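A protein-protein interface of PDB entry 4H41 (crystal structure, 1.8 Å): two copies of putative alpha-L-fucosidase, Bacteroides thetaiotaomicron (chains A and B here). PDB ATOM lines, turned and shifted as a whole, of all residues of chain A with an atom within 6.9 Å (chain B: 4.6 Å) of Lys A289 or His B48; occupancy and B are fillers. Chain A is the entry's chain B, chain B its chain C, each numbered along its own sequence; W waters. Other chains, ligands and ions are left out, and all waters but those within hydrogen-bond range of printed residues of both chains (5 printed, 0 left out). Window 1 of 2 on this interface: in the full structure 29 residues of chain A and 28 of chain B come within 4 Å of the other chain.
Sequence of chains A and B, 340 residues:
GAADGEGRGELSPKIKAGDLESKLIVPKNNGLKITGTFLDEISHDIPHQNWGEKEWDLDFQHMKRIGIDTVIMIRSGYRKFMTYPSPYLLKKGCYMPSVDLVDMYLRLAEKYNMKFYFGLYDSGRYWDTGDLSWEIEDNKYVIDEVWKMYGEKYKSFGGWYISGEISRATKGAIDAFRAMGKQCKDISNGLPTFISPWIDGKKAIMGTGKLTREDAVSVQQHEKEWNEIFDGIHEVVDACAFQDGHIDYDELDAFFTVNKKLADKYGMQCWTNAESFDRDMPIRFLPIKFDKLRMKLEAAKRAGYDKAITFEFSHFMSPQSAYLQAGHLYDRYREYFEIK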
ATOM      1  N   SER A 276      -1.785 -15.750   7.188  1.00  0.00           N
ATOM      2  CA  SER A 276      -3.081 -15.134   7.471  1.00  0.00           C
ATOM      3  C   SER A 276      -3.457 -14.090   6.433  1.00  0.00           C
ATOM      4  O   SER A 276      -4.454 -13.357   6.597  1.00  0.00           O
ATOM      5  CB  SER A 276      -3.084 -14.599   8.902  1.00  0.00           C
ATOM      6  OG  SER A 276      -1.945 -13.829   9.188  1.00  0.00           O
ATOM      7  N   PHE A 277      -2.750 -14.107   5.277  1.00  0.00           N
ATOM      8  CA  PHE A 277      -3.052 -13.288   4.109  1.00  0.00           C
ATOM      9  C   PHE A 277      -3.491 -14.223   2.985  1.00  0.00           C
ATOM     10  O   PHE A 277      -3.148 -15.414   3.010  1.00  0.00           O
ATOM     11  CB  PHE A 277      -1.876 -12.419   3.695  1.00  0.00           C
ATOM     12  CG  PHE A 277      -0.645 -13.193   3.313  1.00  0.00           C
ATOM     13  CD1 PHE A 277       0.257 -13.609   4.278  1.00  0.00           C
ATOM     14  CD2 PHE A 277      -0.435 -13.597   1.999  1.00  0.00           C
ATOM     15  CE1 PHE A 277       1.380 -14.352   3.930  1.00  0.00           C
ATOM     16  CE2 PHE A 277       0.699 -14.324   1.655  1.00  0.00           C
ATOM     17  CZ  PHE A 277       1.623 -14.656   2.623  1.00  0.00           C
ATOM     18  N   ASP A 278      -4.249 -13.704   2.013  1.00  0.00           N
ATOM     19  CA  ASP A 278      -4.794 -14.506   0.951  1.00  0.00           C
ATOM     20  C   ASP A 278      -3.897 -14.501  -0.297  1.00  0.00           C
ATOM     21  O   ASP A 278      -3.690 -13.479  -0.896  1.00  0.00           O
ATOM     22  CB  ASP A 278      -6.219 -13.986   0.601  1.00  0.00           C
ATOM     23  CG  ASP A 278      -7.114 -15.080   0.073  1.00  0.00           C
ATOM     24  OD1 ASP A 278      -6.708 -15.739  -0.908  1.00  0.00           O
ATOM     25  OD2 ASP A 278      -8.238 -15.309   0.676  1.00  0.00           O
ATOM     26  N   MET A 281      -5.934 -14.088  -4.437  1.00  0.00           N
ATOM     27  CA  MET A 281      -6.579 -12.845  -4.842  1.00  0.00           C
ATOM     28  C   MET A 281      -5.689 -11.973  -5.706  1.00  0.00           C
ATOM     29  O   MET A 281      -4.468 -12.023  -5.595  1.00  0.00           O
ATOM     30  CB  MET A 281      -6.979 -12.063  -3.590  1.00  0.00           C
ATOM     31  CG  MET A 281      -7.934 -12.814  -2.677  1.00  0.00           C
ATOM     32  SD  MET A 281      -9.708 -12.891  -3.444  1.00  0.00           S
ATOM     33  CE  MET A 281      -9.940 -14.757  -3.731  1.00  0.00           C
ATOM     34  N   LEU A 286      -4.053  -9.095   1.039  1.00  0.00           N
ATOM     35  CA  LEU A 286      -4.993  -8.683   2.075  1.00  0.00           C
ATOM     36  C   LEU A 286      -5.333  -9.881   2.945  1.00  0.00           C
ATOM     37  O   LEU A 286      -4.899 -11.004   2.643  1.00  0.00           O
ATOM     38  CB  LEU A 286      -6.245  -8.063   1.422  1.00  0.00           C
ATOM     39  CG  LEU A 286      -6.003  -6.675   0.854  1.00  0.00           C
ATOM     40  CD1 LEU A 286      -7.222  -6.235   0.066  1.00  0.00           C
ATOM     41  CD2 LEU A 286      -5.686  -5.680   1.932  1.00  0.00           C
ATOM     42  N   PRO A 287      -6.017  -9.640   4.089  1.00  0.00           N
ATOM     43  CA  PRO A 287      -6.312 -10.759   4.988  1.00  0.00           C
ATOM     44  C   PRO A 287      -7.028 -11.938   4.326  1.00  0.00           C
ATOM     45  O   PRO A 287      -7.877 -11.790   3.417  1.00  0.00           O
ATOM     46  CB  PRO A 287      -7.176 -10.109   6.065  1.00  0.00           C
ATOM     47  CG  PRO A 287      -6.702  -8.659   6.073  1.00  0.00           C
ATOM     48  CD  PRO A 287      -6.483  -8.357   4.670  1.00  0.00           C
ATOM     49  N   ILE A 288      -6.680 -13.141   4.807  1.00  0.00           N
ATOM     50  CA  ILE A 288      -7.261 -14.381   4.307  1.00  0.00           C
ATOM     51  C   ILE A 288      -8.707 -14.555   4.753  1.00  0.00           C
ATOM     52  O   ILE A 288      -9.130 -14.079   5.804  1.00  0.00           O
ATOM     53  CB  ILE A 288      -6.377 -15.589   4.765  1.00  0.00           C
ATOM     54  CG1 ILE A 288      -6.579 -16.810   3.868  1.00  0.00           C
ATOM     55  CG2 ILE A 288      -6.605 -15.939   6.224  1.00  0.00           C
ATOM     56  CD1 ILE A 288      -5.545 -17.917   4.119  1.00  0.00           C
ATOM     57  N   LYS A 289      -9.459 -15.308   3.952  1.00  0.00           N
ATOM     58  CA  LYS A 289     -10.764 -15.808   4.332  1.00  0.00           C
ATOM     59  C   LYS A 289     -10.590 -16.773   5.542  1.00  0.00           C
ATOM     60  O   LYS A 289      -9.800 -17.720   5.482  1.00  0.00           O
ATOM     61  CB  LYS A 289     -11.426 -16.547   3.144  1.00  0.00           C
ATOM     62  CG  LYS A 289     -12.718 -17.246   3.517  1.00  0.00           C
ATOM     63  CD  LYS A 289     -13.374 -17.951   2.323  1.00  0.00           C
ATOM     64  CE  LYS A 289     -13.949 -17.039   1.305  1.00  0.00           C
ATOM     65  NZ  LYS A 289     -14.769 -17.823   0.323  1.00  0.00           N
ATOM     66  N   PHE A 290     -11.299 -16.502   6.634  1.00  0.00           N
ATOM     67  CA  PHE A 290     -11.204 -17.311   7.842  1.00  0.00           C
ATOM     68  C   PHE A 290     -11.265 -18.824   7.558  1.00  0.00           C
ATOM     69  O   PHE A 290     -10.434 -19.579   8.069  1.00  0.00           O
ATOM     70  CB  PHE A 290     -12.314 -16.954   8.834  1.00  0.00           C
ATOM     71  CG  PHE A 290     -12.315 -17.923   9.997  1.00  0.00           C
ATOM     72  CD1 PHE A 290     -11.204 -18.043  10.823  1.00  0.00           C
ATOM     73  CD2 PHE A 290     -13.349 -18.823  10.160  1.00  0.00           C
ATOM     74  CE1 PHE A 290     -11.180 -18.995  11.849  1.00  0.00           C
ATOM     75  CE2 PHE A 290     -13.296 -19.805  11.151  1.00  0.00           C
ATOM     76  CZ  PHE A 290     -12.231 -19.852  12.008  1.00  0.00           C
ATOM     77  N   ASP A 291     -12.221 -19.269   6.752  1.00  0.00           N
ATOM     78  CA  ASP A 291     -12.348 -20.730   6.497  1.00  0.00           C
ATOM     79  C   ASP A 291     -11.113 -21.318   5.873  1.00  0.00           C
ATOM     80  O   ASP A 291     -10.777 -22.452   6.170  1.00  0.00           O
ATOM     81  CB  ASP A 291     -13.577 -21.093   5.651  1.00  0.00           C
ATOM     82  CG  ASP A 291     -14.841 -21.327   6.469  1.00  0.00           C
ATOM     83  OD1 ASP A 291     -14.735 -21.439   7.719  1.00  0.00           O
ATOM     84  OD2 ASP A 291     -15.915 -21.527   5.853  1.00  0.00           O
ATOM     85  N   LYS A 292     -10.350 -20.528   5.100  1.00  0.00           N
ATOM     86  CA  LYS A 292      -9.090 -21.049   4.554  1.00  0.00           C
ATOM     87  C   LYS A 292      -8.063 -21.210   5.658  1.00  0.00           C
ATOM     88  O   LYS A 292      -7.364 -22.239   5.708  1.00  0.00           O
ATOM     89  CB  LYS A 292      -8.547 -20.140   3.457  1.00  0.00           C
ATOM     90  CG  LYS A 292      -9.405 -20.155   2.193  1.00  0.00           C
ATOM     91  CD  LYS A 292      -8.939 -19.100   1.196  1.00  0.00           C
ATOM     92  CE  LYS A 292      -9.846 -19.061  -0.029  1.00  0.00           C
ATOM     93  NZ  LYS A 292      -9.311 -18.091  -1.026  1.00  0.00           N
ATOM     94  N   LEU A 293      -7.952 -20.212   6.548  1.00  0.00           N
ATOM     95  CA  LEU A 293      -7.022 -20.284   7.677  1.00  0.00           C
ATOM     96  C   LEU A 293      -7.420 -21.487   8.563  1.00  0.00           C
ATOM     97  O   LEU A 293      -6.567 -22.263   9.014  1.00  0.00           O
ATOM     98  CB  LEU A 293      -7.045 -19.002   8.497  1.00  0.00           C
ATOM     99  CG  LEU A 293      -6.084 -18.983   9.693  1.00  0.00           C
ATOM    100  CD1 LEU A 293      -4.655 -19.210   9.294  1.00  0.00           C
ATOM    101  CD2 LEU A 293      -6.148 -17.654  10.433  1.00  0.00           C
ATOM    102  N   ARG A 294      -8.722 -21.619   8.810  1.00  0.00           N
ATOM    103  CA  ARG A 294      -9.269 -22.697   9.667  1.00  0.00           C
ATOM    104  C   ARG A 294      -8.845 -24.044   9.083  1.00  0.00           C
ATOM    105  O   ARG A 294      -8.430 -24.913   9.801  1.00  0.00           O
ATOM    106  CB  ARG A 294     -10.809 -22.600   9.764  1.00  0.00           C
ATOM    107  CG  ARG A 294     -11.367 -23.664  10.599  1.00  0.00           C
ATOM    108  CD  ARG A 294     -12.862 -23.705  10.661  1.00  0.00           C
ATOM    109  NE  ARG A 294     -13.515 -23.629   9.374  1.00  0.00           N
ATOM    110  CZ  ARG A 294     -13.713 -24.626   8.518  1.00  0.00           C
ATOM    111  NH1 ARG A 294     -13.313 -25.856   8.811  1.00  0.00           N
ATOM    112  NH2 ARG A 294     -14.362 -24.414   7.390  1.00  0.00           N
ATOM    113  N   GLN A 325     -10.475  -6.018   7.278  1.00  0.00           N
ATOM    114  CA  GLN A 325     -10.827  -7.443   7.160  1.00  0.00           C
ATOM    115  C   GLN A 325     -10.070  -8.262   8.207  1.00  0.00           C
ATOM    116  O   GLN A 325     -10.500  -9.356   8.567  1.00  0.00           O
ATOM    117  CB  GLN A 325     -10.519  -8.001   5.741  1.00  0.00           C
ATOM    118  CG  GLN A 325     -11.045  -7.142   4.575  1.00  0.00           C
ATOM    119  CD  GLN A 325     -10.063  -6.091   4.085  1.00  0.00           C
ATOM    120  OE1 GLN A 325      -9.215  -5.589   4.843  1.00  0.00           O
ATOM    121  NE2 GLN A 325     -10.131  -5.742   2.820  1.00  0.00           N
ATOM    122  N   ALA A 326      -8.938  -7.735   8.683  1.00  0.00           N
ATOM    123  CA  ALA A 326      -8.116  -8.342   9.728  1.00  0.00           C
ATOM    124  C   ALA A 326      -8.817  -8.334  11.083  1.00  0.00           C
ATOM    125  O   ALA A 326      -8.801  -9.355  11.757  1.00  0.00           O
ATOM    126  CB  ALA A 326      -6.783  -7.624   9.852  1.00  0.00           C
ATOM    127  N   LEU A 329     -11.379 -10.887  10.890  1.00  0.00           N
ATOM    128  CA  LEU A 329     -10.730 -12.206  10.972  1.00  0.00           C
ATOM    129  C   LEU A 329     -10.449 -12.574  12.437  1.00  0.00           C
ATOM    130  O   LEU A 329     -10.673 -13.709  12.853  1.00  0.00           O
ATOM    131  CB  LEU A 329      -9.426 -12.238  10.198  1.00  0.00           C
ATOM    132  CG  LEU A 329      -8.653 -13.590  10.203  1.00  0.00           C
ATOM    133  CD1 LEU A 329      -9.519 -14.748   9.805  1.00  0.00           C
ATOM    134  CD2 LEU A 329      -7.493 -13.520   9.192  1.00  0.00           C
ATOM    135  N   ARG A 332     -13.696 -13.761  13.991  1.00  0.00           N
ATOM    136  CA  ARG A 332     -14.058 -15.135  13.543  1.00  0.00           C
ATOM    137  C   ARG A 332     -13.162 -16.171  14.208  1.00  0.00           C
ATOM    138  O   ARG A 332     -13.630 -17.255  14.587  1.00  0.00           O
ATOM    139  CB  ARG A 332     -13.956 -15.274  12.020  1.00  0.00           C
ATOM    140  CG  ARG A 332     -14.804 -14.328  11.177  1.00  0.00           C
ATOM    141  CD  ARG A 332     -16.318 -14.521  11.256  1.00  0.00           C
ATOM    142  NE  ARG A 332     -16.914 -14.062  12.515  1.00  0.00           N
ATOM    143  CZ  ARG A 332     -17.053 -12.796  12.909  1.00  0.00           C
ATOM    144  NH1 ARG A 332     -16.681 -11.789  12.117  1.00  0.00           N
ATOM    145  NH2 ARG A 332     -17.576 -12.523  14.088  1.00  0.00           N
ATOM    146  N   GLU B  41     -20.381 -14.259  -2.658  1.00  0.00           N
ATOM    147  CA  GLU B  41     -20.078 -15.593  -2.118  1.00  0.00           C
ATOM    148  C   GLU B  41     -20.472 -16.620  -3.165  1.00  0.00           C
ATOM    149  O   GLU B  41     -21.614 -16.539  -3.590  1.00  0.00           O
ATOM    150  CB  GLU B  41     -20.900 -15.854  -0.845  1.00  0.00           C
ATOM    151  CG  GLU B  41     -20.563 -14.944   0.309  1.00  0.00           C
ATOM    152  CD  GLU B  41     -19.282 -15.251   1.045  1.00  0.00           C
ATOM    153  OE1 GLU B  41     -18.634 -16.285   0.759  1.00  0.00           O
ATOM    154  OE2 GLU B  41     -18.947 -14.453   1.943  1.00  0.00           O
ATOM    155  N   ILE B  42     -19.632 -17.580  -3.586  1.00  0.00           N
ATOM    156  CA  ILE B  42     -18.190 -17.661  -3.315  1.00  0.00           C
ATOM    157  C   ILE B  42     -17.501 -16.703  -4.284  1.00  0.00           C
ATOM    158  O   ILE B  42     -17.689 -16.834  -5.485  1.00  0.00           O
ATOM    159  CB  ILE B  42     -17.645 -19.089  -3.485  1.00  0.00           C
ATOM    160  CG1 ILE B  42     -18.299 -20.089  -2.519  1.00  0.00           C
ATOM    161  CG2 ILE B  42     -16.117 -19.074  -3.346  1.00  0.00           C
ATOM    162  CD1 ILE B  42     -18.098 -19.804  -1.009  1.00  0.00           C
ATOM    163  N   ILE B  46     -12.408 -11.168  -5.050  1.00  0.00           N
ATOM    164  CA  ILE B  46     -12.521 -10.023  -4.129  1.00  0.00           C
ATOM    165  C   ILE B  46     -12.146 -10.532  -2.723  1.00  0.00           C
ATOM    166  O   ILE B  46     -12.806 -11.434  -2.215  1.00  0.00           O
ATOM    167  CB  ILE B  46     -13.914  -9.416  -4.136  1.00  0.00           C
ATOM    168  CG1 ILE B  46     -14.414  -9.091  -5.586  1.00  0.00           C
ATOM    169  CG2 ILE B  46     -13.958  -8.193  -3.230  1.00  0.00           C
ATOM    170  CD1 ILE B  46     -13.504  -8.113  -6.381  1.00  0.00           C
ATOM    171  N   PRO B  47     -11.146  -9.925  -2.066  1.00  0.00           N
ATOM    172  CA  PRO B  47     -10.729 -10.420  -0.742  1.00  0.00           C
ATOM    173  C   PRO B  47     -11.877 -10.400   0.260  1.00  0.00           C
ATOM    174  O   PRO B  47     -12.744  -9.541   0.227  1.00  0.00           O
ATOM    175  CB  PRO B  47      -9.589  -9.507  -0.344  1.00  0.00           C
ATOM    176  CG  PRO B  47      -8.969  -9.117  -1.664  1.00  0.00           C
ATOM    177  CD  PRO B  47     -10.198  -8.903  -2.570  1.00  0.00           C
ATOM    178  N   HIS B  48     -11.923 -11.428   1.058  1.00  0.00           N
ATOM    179  CA  HIS B  48     -13.012 -11.671   2.003  1.00  0.00           C
ATOM    180  C   HIS B  48     -12.978 -10.680   3.141  1.00  0.00           C
ATOM    181  O   HIS B  48     -11.897 -10.376   3.673  1.00  0.00           O
ATOM    182  CB  HIS B  48     -12.893 -13.100   2.541  1.00  0.00           C
ATOM    183  CG  HIS B  48     -14.127 -13.660   3.217  1.00  0.00           C
ATOM    184  ND1 HIS B  48     -15.306 -13.835   2.541  1.00  0.00           N
ATOM    185  CD2 HIS B  48     -14.283 -14.131   4.483  1.00  0.00           C
ATOM    186  CE1 HIS B  48     -16.152 -14.386   3.398  1.00  0.00           C
ATOM    187  NE2 HIS B  48     -15.589 -14.565   4.592  1.00  0.00           N
ATOM    188  N   GLN B  49     -14.163 -10.191   3.577  1.00  0.00           N
ATOM    189  CA  GLN B  49     -14.193  -9.225   4.691  1.00  0.00           C
ATOM    190  C   GLN B  49     -14.322  -9.900   6.063  1.00  0.00           C
ATOM    191  O   GLN B  49     -14.239  -9.224   7.072  1.00  0.00           O
ATOM    192  CB  GLN B  49     -15.305  -8.192   4.507  1.00  0.00           C
ATOM    193  CG  GLN B  49     -15.134  -7.426   3.214  1.00  0.00           C
ATOM    194  CD  GLN B  49     -15.847  -6.098   3.260  1.00  0.00           C
ATOM    195  OE1 GLN B  49     -15.398  -5.187   3.920  1.00  0.00           O
ATOM    196  NE2 GLN B  49     -16.976  -5.994   2.608  1.00  0.00           N
ATOM    197  N   ASN B  50     -14.530 -11.233   6.114  1.00  0.00           N
ATOM    198  CA  ASN B  50     -14.564 -11.997   7.341  1.00  0.00           C
ATOM    199  C   ASN B  50     -15.717 -11.566   8.235  1.00  0.00           C
ATOM    200  O   ASN B  50     -15.650 -11.662   9.447  1.00  0.00           O
ATOM    201  CB  ASN B  50     -13.195 -11.932   8.074  1.00  0.00           C
ATOM    202  CG  ASN B  50     -12.188 -12.765   7.346  1.00  0.00           C
ATOM    203  OD1 ASN B  50     -12.421 -13.959   7.174  1.00  0.00           O
ATOM    204  ND2 ASN B  50     -11.094 -12.201   6.950  1.00  0.00           N
HETATM  205  O   HOH W   1     -17.314 -18.210   1.943  1.00  0.00           O
HETATM  206  O   HOH W   2      -9.266  -9.428   3.084  1.00  0.00           O
HETATM  207  O   HOH W   3     -11.998  -6.828   0.787  1.00  0.00           O
HETATM  208  O   HOH W   4      -9.448 -12.866   1.351  1.00  0.00           O
HETATM  209  O   HOH W   5     -16.385 -15.895  -0.850  1.00  0.00           O
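The backbone NH of Ile A288 lies within hydrogen-bond range of the backbone carbonyl oxygen of Ser A276 (2.9 Å).
The backbone carbonyl oxygen of Leu A286 sits at hydrogen-bond distance from the backbone NH of Asp A278 (2.8 Å).
The side-chain carboxylate (OD2) of Asp A278 is in hydrogen-bond range of the backbone NH (N) of Lys A289 (3.5 Å).
Water W1 bridges the side-chain carboxylate of Glu B41 (2.6 Å) and the side-chain amino group of Lys A289 (3.0 Å).
Water W2 bridges the backbone carbonyl oxygen (O) of Pro A287 (2.8 Å) and the backbone carbonyl oxygen (O) of His B48 (2.9 Å).
Water W5 lies within hydrogen-bond range of NZ of Lys A289 and OE1 of Glu B41.
Water W4 lies within hydrogen-bond range of OD2 of Asp A278 (2.8 Å), O of Pro A287 (2.8 Å) and N of His B48 (2.9 Å).
Water W3 bridges the backbone carbonyl oxygen (O) of Pro B47 (2.9 Å) and the side-chain amide nitrogen (NE2) of Gln A325 (3.0 Å).
SD of Met A281 sits close to N of Ile B46.
The backbone carbonyl oxygen of Ile A288 lies within hydrogen-bond range of the side-chain amide nitrogen of Asn B50 (2.9 Å).
The side-chain amide oxygen of Asn B50 is in hydrogen-bond range of the backbone NH of Phe A290 (2.8 Å).
O of Gln A325 is in hydrogen-bond range of ND2 of Asn B50 (3.3 Å).
The guanidinium group of Arg A332 sits at hydrogen-bond distance from the backbone carbonyl oxygen of Asn B50.
SD of Met A281 lies close to N of Pro B47, at 3.6 Å.
No position is printed for both chains.
Among the printed residues, merely in contact across the chains: Gln A325 with His B48 (3.4 Å), Leu A329 with Asn B50 (3.5 Å), Lys A289 with His B48 (3.6 Å), Lys A289 with Asn B50 (3.7 Å), Gln A325 with Gln B49 (3.8 Å) and Leu A286 with Pro B47 (3.8 Å).
Printed residues of chain B that touch a printed residue of chain A: Ile B46, Pro B47, His B48, Gln B49 and Asn B50.
Hydrophobic or aromatic side chains of chain A that line the printed part of chain B: Met A281, Leu A286, Phe A290 and Leu A329.
Among the printed residues, no Asp or Glu carboxylate lies within 4 Å of a Lys or Arg side-chain nitrogen of the other chain.
Lys A289 touches just these residues of chain B: His B48 (3.6 Å) and Asn B50 (3.7 Å).
Of the printed residues of chain B, Phe A290 touches Asn B50 (2.8 Å).
Leu A293 touches none of the printed residues of chain B.
Of the printed residues of chain A, Ile B46 touches Met A281 (3.5 Å).
His B48 touches just these residues of chain A: Lys A289 (3.6 Å) and Gln A325 (3.4 Å).
The nearest residue of chain B that does not touch Lys A289 is Ile B42 (4.1 Å).
The nearest residue of chain A that does not touch His B48 is Pro A287 (4.3 Å).
The nearest printed residue of chain A that does not touch Gln B49 is Leu A329 (5.1 Å).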
